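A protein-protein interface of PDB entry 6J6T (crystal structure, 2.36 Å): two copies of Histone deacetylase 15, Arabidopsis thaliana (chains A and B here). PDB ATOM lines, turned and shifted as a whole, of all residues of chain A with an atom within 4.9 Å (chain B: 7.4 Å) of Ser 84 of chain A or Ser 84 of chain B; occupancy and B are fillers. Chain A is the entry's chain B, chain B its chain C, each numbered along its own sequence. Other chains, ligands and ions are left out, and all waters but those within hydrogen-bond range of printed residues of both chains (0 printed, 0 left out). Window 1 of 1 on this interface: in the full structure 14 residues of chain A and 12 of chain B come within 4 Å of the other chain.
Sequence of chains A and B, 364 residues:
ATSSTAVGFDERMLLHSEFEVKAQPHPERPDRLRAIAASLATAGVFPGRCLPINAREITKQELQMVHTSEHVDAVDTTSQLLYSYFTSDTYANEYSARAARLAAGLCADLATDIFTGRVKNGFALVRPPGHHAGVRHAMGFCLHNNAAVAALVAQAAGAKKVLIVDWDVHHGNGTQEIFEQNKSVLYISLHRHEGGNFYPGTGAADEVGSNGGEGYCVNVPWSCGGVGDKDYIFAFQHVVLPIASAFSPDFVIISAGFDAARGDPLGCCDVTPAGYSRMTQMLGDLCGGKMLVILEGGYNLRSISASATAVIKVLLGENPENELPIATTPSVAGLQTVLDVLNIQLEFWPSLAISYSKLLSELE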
ATOM      1  N   THR A  78     -10.499  -3.036  23.145  1.00  0.00           N
ATOM      2  CA  THR A  78     -10.782  -2.019  24.149  1.00  0.00           C
ATOM      3  C   THR A  78     -11.991  -2.379  25.006  1.00  0.00           C
ATOM      4  O   THR A  78     -12.150  -1.807  26.088  1.00  0.00           O
ATOM      5  CB  THR A  78     -10.989  -0.644  23.490  1.00  0.00           C
ATOM      6  OG1 THR A  78     -12.173  -0.653  22.681  1.00  0.00           O
ATOM      7  CG2 THR A  78      -9.789  -0.281  22.631  1.00  0.00           C
ATOM      8  N   LEU A  81     -10.847  -3.356  28.592  1.00  0.00           N
ATOM      9  CA  LEU A  81     -10.059  -2.422  29.383  1.00  0.00           C
ATOM     10  C   LEU A  81     -10.995  -1.429  30.049  1.00  0.00           C
ATOM     11  O   LEU A  81     -12.088  -1.167  29.550  1.00  0.00           O
ATOM     12  CB  LEU A  81      -9.045  -1.673  28.508  1.00  0.00           C
ATOM     13  CG  LEU A  81      -8.163  -2.551  27.606  1.00  0.00           C
ATOM     14  CD1 LEU A  81      -7.450  -1.753  26.521  1.00  0.00           C
ATOM     15  CD2 LEU A  81      -7.139  -3.341  28.436  1.00  0.00           C
ATOM     16  N   LEU A  82     -10.582  -0.875  31.183  1.00  0.00           N
ATOM     17  CA  LEU A  82     -11.426   0.127  31.823  1.00  0.00           C
ATOM     18  C   LEU A  82     -11.559   1.365  30.935  1.00  0.00           C
ATOM     19  O   LEU A  82     -12.671   1.826  30.662  1.00  0.00           O
ATOM     20  CB  LEU A  82     -10.868   0.491  33.198  1.00  0.00           C
ATOM     21  CG  LEU A  82     -11.670   1.598  33.887  1.00  0.00           C
ATOM     22  CD1 LEU A  82     -13.085   1.141  34.119  1.00  0.00           C
ATOM     23  CD2 LEU A  82     -11.014   1.964  35.195  1.00  0.00           C
ATOM     24  N   TYR A  83     -10.438   1.918  30.472  1.00  0.00           N
ATOM     25  CA  TYR A  83     -10.500   2.926  29.417  1.00  0.00           C
ATOM     26  C   TYR A  83      -9.185   2.922  28.666  1.00  0.00           C
ATOM     27  O   TYR A  83      -8.179   2.402  29.149  1.00  0.00           O
ATOM     28  CB  TYR A  83     -10.829   4.333  29.935  1.00  0.00           C
ATOM     29  CG  TYR A  83      -9.877   4.945  30.949  1.00  0.00           C
ATOM     30  CD1 TYR A  83     -10.010   4.669  32.308  1.00  0.00           C
ATOM     31  CD2 TYR A  83      -8.884   5.840  30.558  1.00  0.00           C
ATOM     32  CE1 TYR A  83      -9.157   5.242  33.258  1.00  0.00           C
ATOM     33  CE2 TYR A  83      -8.016   6.433  31.502  1.00  0.00           C
ATOM     34  CZ  TYR A  83      -8.166   6.123  32.847  1.00  0.00           C
ATOM     35  OH  TYR A  83      -7.334   6.684  33.790  1.00  0.00           O
ATOM     36  N   SER A  84      -9.211   3.492  27.465  1.00  0.00           N
ATOM     37  CA  SER A  84      -8.026   3.489  26.631  1.00  0.00           C
ATOM     38  C   SER A  84      -8.036   4.670  25.678  1.00  0.00           C
ATOM     39  O   SER A  84      -9.063   5.304  25.442  1.00  0.00           O
ATOM     40  CB  SER A  84      -7.891   2.172  25.856  1.00  0.00           C
ATOM     41  OG  SER A  84      -9.164   1.664  25.502  1.00  0.00           O
ATOM     42  N   TYR A  85      -6.862   4.939  25.119  1.00  0.00           N
ATOM     43  CA  TYR A  85      -6.652   6.034  24.198  1.00  0.00           C
ATOM     44  C   TYR A  85      -5.943   5.527  22.956  1.00  0.00           C
ATOM     45  O   TYR A  85      -4.875   4.914  23.051  1.00  0.00           O
ATOM     46  CB  TYR A  85      -5.852   7.157  24.878  1.00  0.00           C
ATOM     47  CG  TYR A  85      -6.753   8.015  25.726  1.00  0.00           C
ATOM     48  CD1 TYR A  85      -7.415   9.103  25.170  1.00  0.00           C
ATOM     49  CD2 TYR A  85      -6.993   7.707  27.058  1.00  0.00           C
ATOM     50  CE1 TYR A  85      -8.263   9.875  25.917  1.00  0.00           C
ATOM     51  CE2 TYR A  85      -7.840   8.483  27.825  1.00  0.00           C
ATOM     52  CZ  TYR A  85      -8.472   9.570  27.245  1.00  0.00           C
ATOM     53  OH  TYR A  85      -9.323  10.362  27.980  1.00  0.00           O
ATOM     54  N   PHE A  86      -6.544   5.782  21.784  1.00  0.00           N
ATOM     55  CA  PHE A  86      -5.838   5.516  20.534  1.00  0.00           C
ATOM     56  C   PHE A  86      -4.874   6.648  20.195  1.00  0.00           C
ATOM     57  O   PHE A  86      -3.792   6.408  19.672  1.00  0.00           O
ATOM     58  CB  PHE A  86      -6.829   5.323  19.396  1.00  0.00           C
ATOM     59  CG  PHE A  86      -7.770   4.166  19.597  1.00  0.00           C
ATOM     60  CD1 PHE A  86      -7.411   2.895  19.202  1.00  0.00           C
ATOM     61  CD2 PHE A  86      -9.026   4.363  20.142  1.00  0.00           C
ATOM     62  CE1 PHE A  86      -8.276   1.828  19.380  1.00  0.00           C
ATOM     63  CE2 PHE A  86      -9.895   3.301  20.315  1.00  0.00           C
ATOM     64  CZ  PHE A  86      -9.513   2.031  19.939  1.00  0.00           C
ATOM     65  N   THR A  90      -8.650  10.699  21.263  1.00  0.00           N
ATOM     66  CA  THR A  90      -9.576   9.649  20.836  1.00  0.00           C
ATOM     67  C   THR A  90      -9.608   8.555  21.905  1.00  0.00           C
ATOM     68  O   THR A  90      -8.700   7.717  21.987  1.00  0.00           O
ATOM     69  CB  THR A  90      -9.190   9.099  19.462  1.00  0.00           C
ATOM     70  OG1 THR A  90      -9.117  10.177  18.524  1.00  0.00           O
ATOM     71  CG2 THR A  90     -10.248   8.085  18.951  1.00  0.00           C
ATOM     72  N   TYR A  91     -10.670   8.557  22.708  1.00  0.00           N
ATOM     73  CA  TYR A  91     -10.786   7.702  23.874  1.00  0.00           C
ATOM     74  C   TYR A  91     -11.623   6.459  23.556  1.00  0.00           C
ATOM     75  O   TYR A  91     -12.278   6.360  22.522  1.00  0.00           O
ATOM     76  CB  TYR A  91     -11.420   8.477  25.032  1.00  0.00           C
ATOM     77  CG  TYR A  91     -12.827   8.953  24.706  1.00  0.00           C
ATOM     78  CD1 TYR A  91     -13.922   8.083  24.806  1.00  0.00           C
ATOM     79  CD2 TYR A  91     -13.060  10.268  24.281  1.00  0.00           C
ATOM     80  CE1 TYR A  91     -15.223   8.510  24.498  1.00  0.00           C
ATOM     81  CE2 TYR A  91     -14.351  10.705  23.968  1.00  0.00           C
ATOM     82  CZ  TYR A  91     -15.426   9.813  24.088  1.00  0.00           C
ATOM     83  OH  TYR A  91     -16.695  10.223  23.772  1.00  0.00           O
ATOM     84  N   ALA A  92     -11.611   5.513  24.492  1.00  0.00           N
ATOM     85  CA  ALA A  92     -12.535   4.390  24.458  1.00  0.00           C
ATOM     86  C   ALA A  92     -12.812   3.956  25.887  1.00  0.00           C
ATOM     87  O   ALA A  92     -11.979   4.145  26.782  1.00  0.00           O
ATOM     88  CB  ALA A  92     -11.993   3.216  23.636  1.00  0.00           C
ATOM     89  N   PHE B  19       1.497   7.493  31.642  1.00  0.00           N
ATOM     90  CA  PHE B  19       1.585   8.179  30.363  1.00  0.00           C
ATOM     91  C   PHE B  19       2.181   9.575  30.517  1.00  0.00           C
ATOM     92  O   PHE B  19       2.941  10.034  29.652  1.00  0.00           O
ATOM     93  CB  PHE B  19       0.188   8.226  29.738  1.00  0.00           C
ATOM     94  CG  PHE B  19       0.069   9.127  28.544  1.00  0.00           C
ATOM     95  CD1 PHE B  19       0.761   8.849  27.382  1.00  0.00           C
ATOM     96  CD2 PHE B  19      -0.774  10.223  28.576  1.00  0.00           C
ATOM     97  CE1 PHE B  19       0.631   9.660  26.285  1.00  0.00           C
ATOM     98  CE2 PHE B  19      -0.910  11.038  27.482  1.00  0.00           C
ATOM     99  CZ  PHE B  19      -0.206  10.758  26.330  1.00  0.00           C
ATOM    100  N   ALA B  74      -5.601  -9.322  25.570  1.00  0.00           N
ATOM    101  CA  ALA B  74      -5.814  -7.962  26.042  1.00  0.00           C
ATOM    102  C   ALA B  74      -4.490  -7.278  26.382  1.00  0.00           C
ATOM    103  O   ALA B  74      -4.273  -6.115  26.014  1.00  0.00           O
ATOM    104  CB  ALA B  74      -6.741  -7.966  27.264  1.00  0.00           C
ATOM    105  N   VAL B  75      -3.584  -7.983  27.068  1.00  0.00           N
ATOM    106  CA  VAL B  75      -2.351  -7.337  27.511  1.00  0.00           C
ATOM    107  C   VAL B  75      -1.520  -6.883  26.319  1.00  0.00           C
ATOM    108  O   VAL B  75      -1.017  -5.755  26.292  1.00  0.00           O
ATOM    109  CB  VAL B  75      -1.553  -8.256  28.444  1.00  0.00           C
ATOM    110  CG1 VAL B  75      -0.154  -7.714  28.625  1.00  0.00           C
ATOM    111  CG2 VAL B  75      -2.283  -8.391  29.806  1.00  0.00           C
ATOM    112  N   THR B  77      -2.470  -6.393  23.104  1.00  0.00           N
ATOM    113  CA  THR B  77      -3.029  -5.396  22.206  1.00  0.00           C
ATOM    114  C   THR B  77      -2.806  -3.977  22.728  1.00  0.00           C
ATOM    115  O   THR B  77      -2.819  -3.041  21.927  1.00  0.00           O
ATOM    116  CB  THR B  77      -4.513  -5.687  21.963  1.00  0.00           C
ATOM    117  OG1 THR B  77      -4.624  -6.958  21.311  1.00  0.00           O
ATOM    118  CG2 THR B  77      -5.142  -4.643  21.051  1.00  0.00           C
ATOM    119  N   THR B  78      -2.518  -3.798  24.030  1.00  0.00           N
ATOM    120  CA  THR B  78      -2.212  -2.460  24.539  1.00  0.00           C
ATOM    121  C   THR B  78      -0.955  -1.872  23.917  1.00  0.00           C
ATOM    122  O   THR B  78      -0.734  -0.663  24.034  1.00  0.00           O
ATOM    123  CB  THR B  78      -2.034  -2.433  26.067  1.00  0.00           C
ATOM    124  OG1 THR B  78      -0.820  -3.111  26.439  1.00  0.00           O
ATOM    125  CG2 THR B  78      -3.213  -3.062  26.764  1.00  0.00           C
ATOM    126  N   SER B  79      -0.113  -2.687  23.285  1.00  0.00           N
ATOM    127  CA  SER B  79       1.000  -2.095  22.559  1.00  0.00           C
ATOM    128  C   SER B  79       0.539  -1.335  21.323  1.00  0.00           C
ATOM    129  O   SER B  79       1.329  -0.587  20.746  1.00  0.00           O
ATOM    130  CB  SER B  79       2.032  -3.162  22.162  1.00  0.00           C
ATOM    131  OG  SER B  79       1.521  -4.011  21.154  1.00  0.00           O
ATOM    132  N   LEU B  81      -2.021   0.860  21.489  1.00  0.00           N
ATOM    133  CA  LEU B  81      -2.701   2.048  21.981  1.00  0.00           C
ATOM    134  C   LEU B  81      -1.683   3.027  22.558  1.00  0.00           C
ATOM    135  O   LEU B  81      -0.573   2.656  22.938  1.00  0.00           O
ATOM    136  CB  LEU B  81      -3.736   1.667  23.048  1.00  0.00           C
ATOM    137  CG  LEU B  81      -4.595   0.430  22.736  1.00  0.00           C
ATOM    138  CD1 LEU B  81      -5.377  -0.064  23.975  1.00  0.00           C
ATOM    139  CD2 LEU B  81      -5.536   0.700  21.554  1.00  0.00           C
ATOM    140  N   LEU B  82      -2.069   4.294  22.621  1.00  0.00           N
ATOM    141  CA  LEU B  82      -1.218   5.287  23.263  1.00  0.00           C
ATOM    142  C   LEU B  82      -1.061   4.987  24.757  1.00  0.00           C
ATOM    143  O   LEU B  82       0.063   4.884  25.271  1.00  0.00           O
ATOM    144  CB  LEU B  82      -1.790   6.683  23.031  1.00  0.00           C
ATOM    145  CG  LEU B  82      -0.943   7.881  23.479  1.00  0.00           C
ATOM    146  CD1 LEU B  82       0.403   7.848  22.751  1.00  0.00           C
ATOM    147  CD2 LEU B  82      -1.684   9.183  23.206  1.00  0.00           C
ATOM    148  N   TYR B  83      -2.177   4.848  25.476  1.00  0.00           N
ATOM    149  CA  TYR B  83      -2.106   4.355  26.845  1.00  0.00           C
ATOM    150  C   TYR B  83      -3.441   3.742  27.228  1.00  0.00           C
ATOM    151  O   TYR B  83      -4.466   4.005  26.598  1.00  0.00           O
ATOM    152  CB  TYR B  83      -1.677   5.448  27.838  1.00  0.00           C
ATOM    153  CG  TYR B  83      -2.596   6.639  28.039  1.00  0.00           C
ATOM    154  CD1 TYR B  83      -2.664   7.668  27.104  1.00  0.00           C
ATOM    155  CD2 TYR B  83      -3.348   6.764  29.203  1.00  0.00           C
ATOM    156  CE1 TYR B  83      -3.485   8.774  27.309  1.00  0.00           C
ATOM    157  CE2 TYR B  83      -4.168   7.877  29.426  1.00  0.00           C
ATOM    158  CZ  TYR B  83      -4.225   8.875  28.481  1.00  0.00           C
ATOM    159  OH  TYR B  83      -5.038   9.966  28.691  1.00  0.00           O
ATOM    160  N   SER B  84      -3.416   2.899  28.262  1.00  0.00           N
ATOM    161  CA  SER B  84      -4.645   2.231  28.656  1.00  0.00           C
ATOM    162  C   SER B  84      -4.626   1.903  30.137  1.00  0.00           C
ATOM    163  O   SER B  84      -3.584   1.926  30.791  1.00  0.00           O
ATOM    164  CB  SER B  84      -4.894   0.950  27.846  1.00  0.00           C
ATOM    165  OG  SER B  84      -3.696   0.304  27.532  1.00  0.00           O
ATOM    166  N   TYR B  85      -5.817   1.583  30.655  1.00  0.00           N
ATOM    167  CA  TYR B  85      -5.990   1.214  32.050  1.00  0.00           C
ATOM    168  C   TYR B  85      -6.806  -0.061  32.109  1.00  0.00           C
ATOM    169  O   TYR B  85      -7.917  -0.114  31.577  1.00  0.00           O
ATOM    170  CB  TYR B  85      -6.656   2.347  32.837  1.00  0.00           C
ATOM    171  CG  TYR B  85      -5.646   3.379  33.277  1.00  0.00           C
ATOM    172  CD1 TYR B  85      -5.236   4.393  32.416  1.00  0.00           C
ATOM    173  CD2 TYR B  85      -5.054   3.304  34.535  1.00  0.00           C
ATOM    174  CE1 TYR B  85      -4.275   5.326  32.812  1.00  0.00           C
ATOM    175  CE2 TYR B  85      -4.093   4.228  34.935  1.00  0.00           C
ATOM    176  CZ  TYR B  85      -3.711   5.239  34.069  1.00  0.00           C
ATOM    177  OH  TYR B  85      -2.770   6.160  34.470  1.00  0.00           O
ATOM    178  N   PHE B  86      -6.231  -1.102  32.711  1.00  0.00           N
ATOM    179  CA  PHE B  86      -7.001  -2.306  32.984  1.00  0.00           C
ATOM    180  C   PHE B  86      -7.970  -2.075  34.130  1.00  0.00           C
ATOM    181  O   PHE B  86      -9.086  -2.594  34.125  1.00  0.00           O
ATOM    182  CB  PHE B  86      -6.067  -3.465  33.311  1.00  0.00           C
ATOM    183  CG  PHE B  86      -5.080  -3.767  32.239  1.00  0.00           C
ATOM    184  CD1 PHE B  86      -5.410  -4.617  31.204  1.00  0.00           C
ATOM    185  CD2 PHE B  86      -3.803  -3.220  32.278  1.00  0.00           C
ATOM    186  CE1 PHE B  86      -4.497  -4.899  30.194  1.00  0.00           C
ATOM    187  CE2 PHE B  86      -2.878  -3.506  31.273  1.00  0.00           C
ATOM    188  CZ  PHE B  86      -3.229  -4.349  30.234  1.00  0.00           C
ATOM    189  N   THR B  87      -7.539  -1.328  35.136  1.00  0.00           N
ATOM    190  CA  THR B  87      -8.332  -0.959  36.291  1.00  0.00           C
ATOM    191  C   THR B  87      -7.919   0.454  36.642  1.00  0.00           C
ATOM    192  O   THR B  87      -7.025   1.015  36.003  1.00  0.00           O
ATOM    193  CB  THR B  87      -8.071  -1.863  37.497  1.00  0.00           C
ATOM    194  OG1 THR B  87      -6.716  -1.651  37.928  1.00  0.00           O
ATOM    195  CG2 THR B  87      -8.288  -3.335  37.161  1.00  0.00           C
ATOM    196  N   THR B  90      -4.032   0.243  37.377  1.00  0.00           N
ATOM    197  CA  THR B  90      -3.142  -0.607  36.587  1.00  0.00           C
ATOM    198  C   THR B  90      -3.102  -0.051  35.173  1.00  0.00           C
ATOM    199  O   THR B  90      -4.079  -0.178  34.426  1.00  0.00           O
ATOM    200  CB  THR B  90      -3.612  -2.066  36.594  1.00  0.00           C
ATOM    201  OG1 THR B  90      -3.840  -2.485  37.943  1.00  0.00           O
ATOM    202  CG2 THR B  90      -2.569  -2.971  35.987  1.00  0.00           C
ATOM    203  N   TYR B  91      -1.981   0.569  34.816  1.00  0.00           N
ATOM    204  CA  TYR B  91      -1.788   1.245  33.541  1.00  0.00           C
ATOM    205  C   TYR B  91      -0.967   0.381  32.596  1.00  0.00           C
ATOM    206  O   TYR B  91      -0.305  -0.577  33.003  1.00  0.00           O
ATOM    207  CB  TYR B  91      -1.072   2.590  33.720  1.00  0.00           C
ATOM    208  CG  TYR B  91       0.310   2.451  34.321  1.00  0.00           C
ATOM    209  CD1 TYR B  91       1.405   2.073  33.535  1.00  0.00           C
ATOM    210  CD2 TYR B  91       0.526   2.683  35.680  1.00  0.00           C
ATOM    211  CE1 TYR B  91       2.662   1.927  34.078  1.00  0.00           C
ATOM    212  CE2 TYR B  91       1.794   2.550  36.231  1.00  0.00           C
ATOM    213  CZ  TYR B  91       2.853   2.166  35.419  1.00  0.00           C
ATOM    214  OH  TYR B  91       4.109   2.013  35.947  1.00  0.00           O
ATOM    215  N   ALA B  92      -0.995   0.775  31.325  1.00  0.00           N
ATOM    216  CA  ALA B  92      -0.117   0.277  30.280  1.00  0.00           C
ATOM    217  C   ALA B  92       0.142   1.423  29.303  1.00  0.00           C
ATOM    218  O   ALA B  92      -0.733   2.269  29.079  1.00  0.00           O
ATOM    219  CB  ALA B  92      -0.731  -0.926  29.533  1.00  0.00           C
ATOM    220  N   ASN B  93       1.347   1.449  28.729  1.00  0.00           N
ATOM    221  CA  ASN B  93       1.618   2.256  27.548  1.00  0.00           C
ATOM    222  C   ASN B  93       2.022   1.316  26.396  1.00  0.00           C
ATOM    223  O   ASN B  93       1.860   0.098  26.496  1.00  0.00           O
ATOM    224  CB  ASN B  93       2.651   3.340  27.876  1.00  0.00           C
ATOM    225  CG  ASN B  93       4.029   2.776  28.245  1.00  0.00           C
ATOM    226  OD1 ASN B  93       4.351   1.617  27.969  1.00  0.00           O
ATOM    227  ND2 ASN B  93       4.859   3.619  28.866  1.00  0.00           N
ATOM    228  N   GLU B  94       2.541   1.895  25.298  1.00  0.00           N
ATOM    229  CA  GLU B  94       2.963   1.110  24.128  1.00  0.00           C
ATOM    230  C   GLU B  94       3.936  -0.011  24.467  1.00  0.00           C
ATOM    231  O   GLU B  94       4.032  -0.991  23.717  1.00  0.00           O
ATOM    232  CB  GLU B  94       3.718   1.962  23.111  1.00  0.00           C
ATOM    233  CG  GLU B  94       3.017   3.022  22.376  1.00  0.00           C
ATOM    234  CD  GLU B  94       4.018   4.087  21.961  1.00  0.00           C
ATOM    235  OE1 GLU B  94       3.895   5.229  22.459  1.00  0.00           O
ATOM    236  OE2 GLU B  94       4.944   3.768  21.171  1.00  0.00           O
ATOM    237  N   SER B  96       4.325  -1.637  27.500  1.00  0.00           N
ATOM    238  CA  SER B  96       4.008  -2.422  28.685  1.00  0.00           C
ATOM    239  C   SER B  96       3.955  -3.906  28.362  1.00  0.00           C
ATOM    240  O   SER B  96       4.440  -4.733  29.143  1.00  0.00           O
ATOM    241  CB  SER B  96       2.690  -1.948  29.271  1.00  0.00           C
ATOM    242  OG  SER B  96       2.847  -0.688  29.917  1.00  0.00           O
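Leu 81 of chain A touches Leu 81 of chain B. Ser 84 of chain B touches Leu 81 of chain A. Tyr 85 of chain B touches Leu 81 of chain A (O to CB, 3.6 Å). Leu 82 of chain A touches Phe 86 of chain B (CB to O, 3.7 Å). Leu 82 of chain A touches Thr 87 of chain B (CD2 to C, 3.7 Å). CA of Ser 84 of chain B touches O of Tyr 83 of chain A, 3.6 Å away. CB of Ser 84 of chain A touches CD1 of Leu 81 of chain B (3.9 Å). Ser 84 of chain A touches Ser 84 of chain B (CB to CB, 3.8 Å). O of Tyr 85 of chain A touches CB of Leu 81 of chain B (3.4 Å). Phe 86 of chain A touches Leu 82 of chain B (O to CB, 3.9 Å).
Ser 84 of chain A touches just these residues of chain B: Leu 81 (3.9 Å), Tyr 83 (3.6 Å) and Ser 84 (3.8 Å). Printed residues of chain B within 4 Å of Tyr 85 of chain A: Leu 81, Leu 82 and Tyr 83. Printed residues of chain A within 4 Å of Leu 82 of chain B: Tyr 85 and Phe 86. Ser 84 of chain B touches just these residues of chain A: Leu 81, Tyr 83 and Ser 84. The nearest residue of chain B that does not touch Ser 84 of chain A is Tyr 85 of chain B (5.0 Å). The nearest printed residue of chain A that does not touch Ser 84 of chain B is Tyr 85 of chain A (5.0 Å).
O of Ser 84 of chain A is in hydrogen-bond range of N of Ala 92 of chain A (2.7 Å). The backbone NH (N) of Ser 84 of chain B is in hydrogen-bond range of the backbone carbonyl oxygen (O) of Ala 92 of chain B (2.9 Å). The side-chain hydroxyl of Thr 90 of chain B lies within hydrogen-bond range of the side-chain hydroxyl of Thr 87 of chain B, 3.0 Å away.
Of the 19 printed residues of chain B, 7 touch a printed residue of chain A. Hydrophobic or aromatic side chains of chain B that line the printed part of chain A: Leu 81, Leu 82, Tyr 83, Tyr 85 and Phe 86. Along chain B the printed residues that touch a printed residue of chain A span positions 81 to 87. Among the printed residues, 17 pairs touch across the chains. Among the printed residues, no Asp or Glu carboxylate lies within 4 Å of a Lys or Arg side-chain nitrogen of the other chain.
Leu 81 of chain A touches Tyr 85 of chain B, and with the chains exchanged Tyr 85 of chain A touches Leu 81 of chain B. Leu 82 of chain A touches Tyr 85 of chain B, and with the chains exchanged Tyr 85 of chain A touches Leu 82 of chain B. Tyr 83 of chain A touches Ser 84 of chain B, and with the chains exchanged Ser 84 of chain A touches Tyr 83 of chain B. Tyr 83 of chain A touches Tyr 85 of chain B, and with the chains exchanged Tyr 85 of chain A touches Tyr 83 of chain B. Positions printed for both chains: 78, 81, 82, 83, 84, 85, 86, 90, 91 and 92. Of the 17 pairs that touch across the chains among the printed residues, 16 have their exchanged pair printed and touching as well.
The backbone carbonyl oxygen of Tyr 85 of chain B sits at hydrogen-bond distance from the backbone NH of Leu 82 of chain A, at 2.8 Å. The backbone carbonyl oxygen of Tyr 83 of chain A lies within hydrogen-bond range of the backbone NH of Tyr 85 of chain B, 2.9 Å away. The backbone NH of Leu 82 of chain B lies within hydrogen-bond range of the backbone carbonyl oxygen of Tyr 85 of chain A (2.9 Å). N of Tyr 85 of chain A is in hydrogen-bond range of O of Tyr 83 of chain B, 3.0 Å away.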
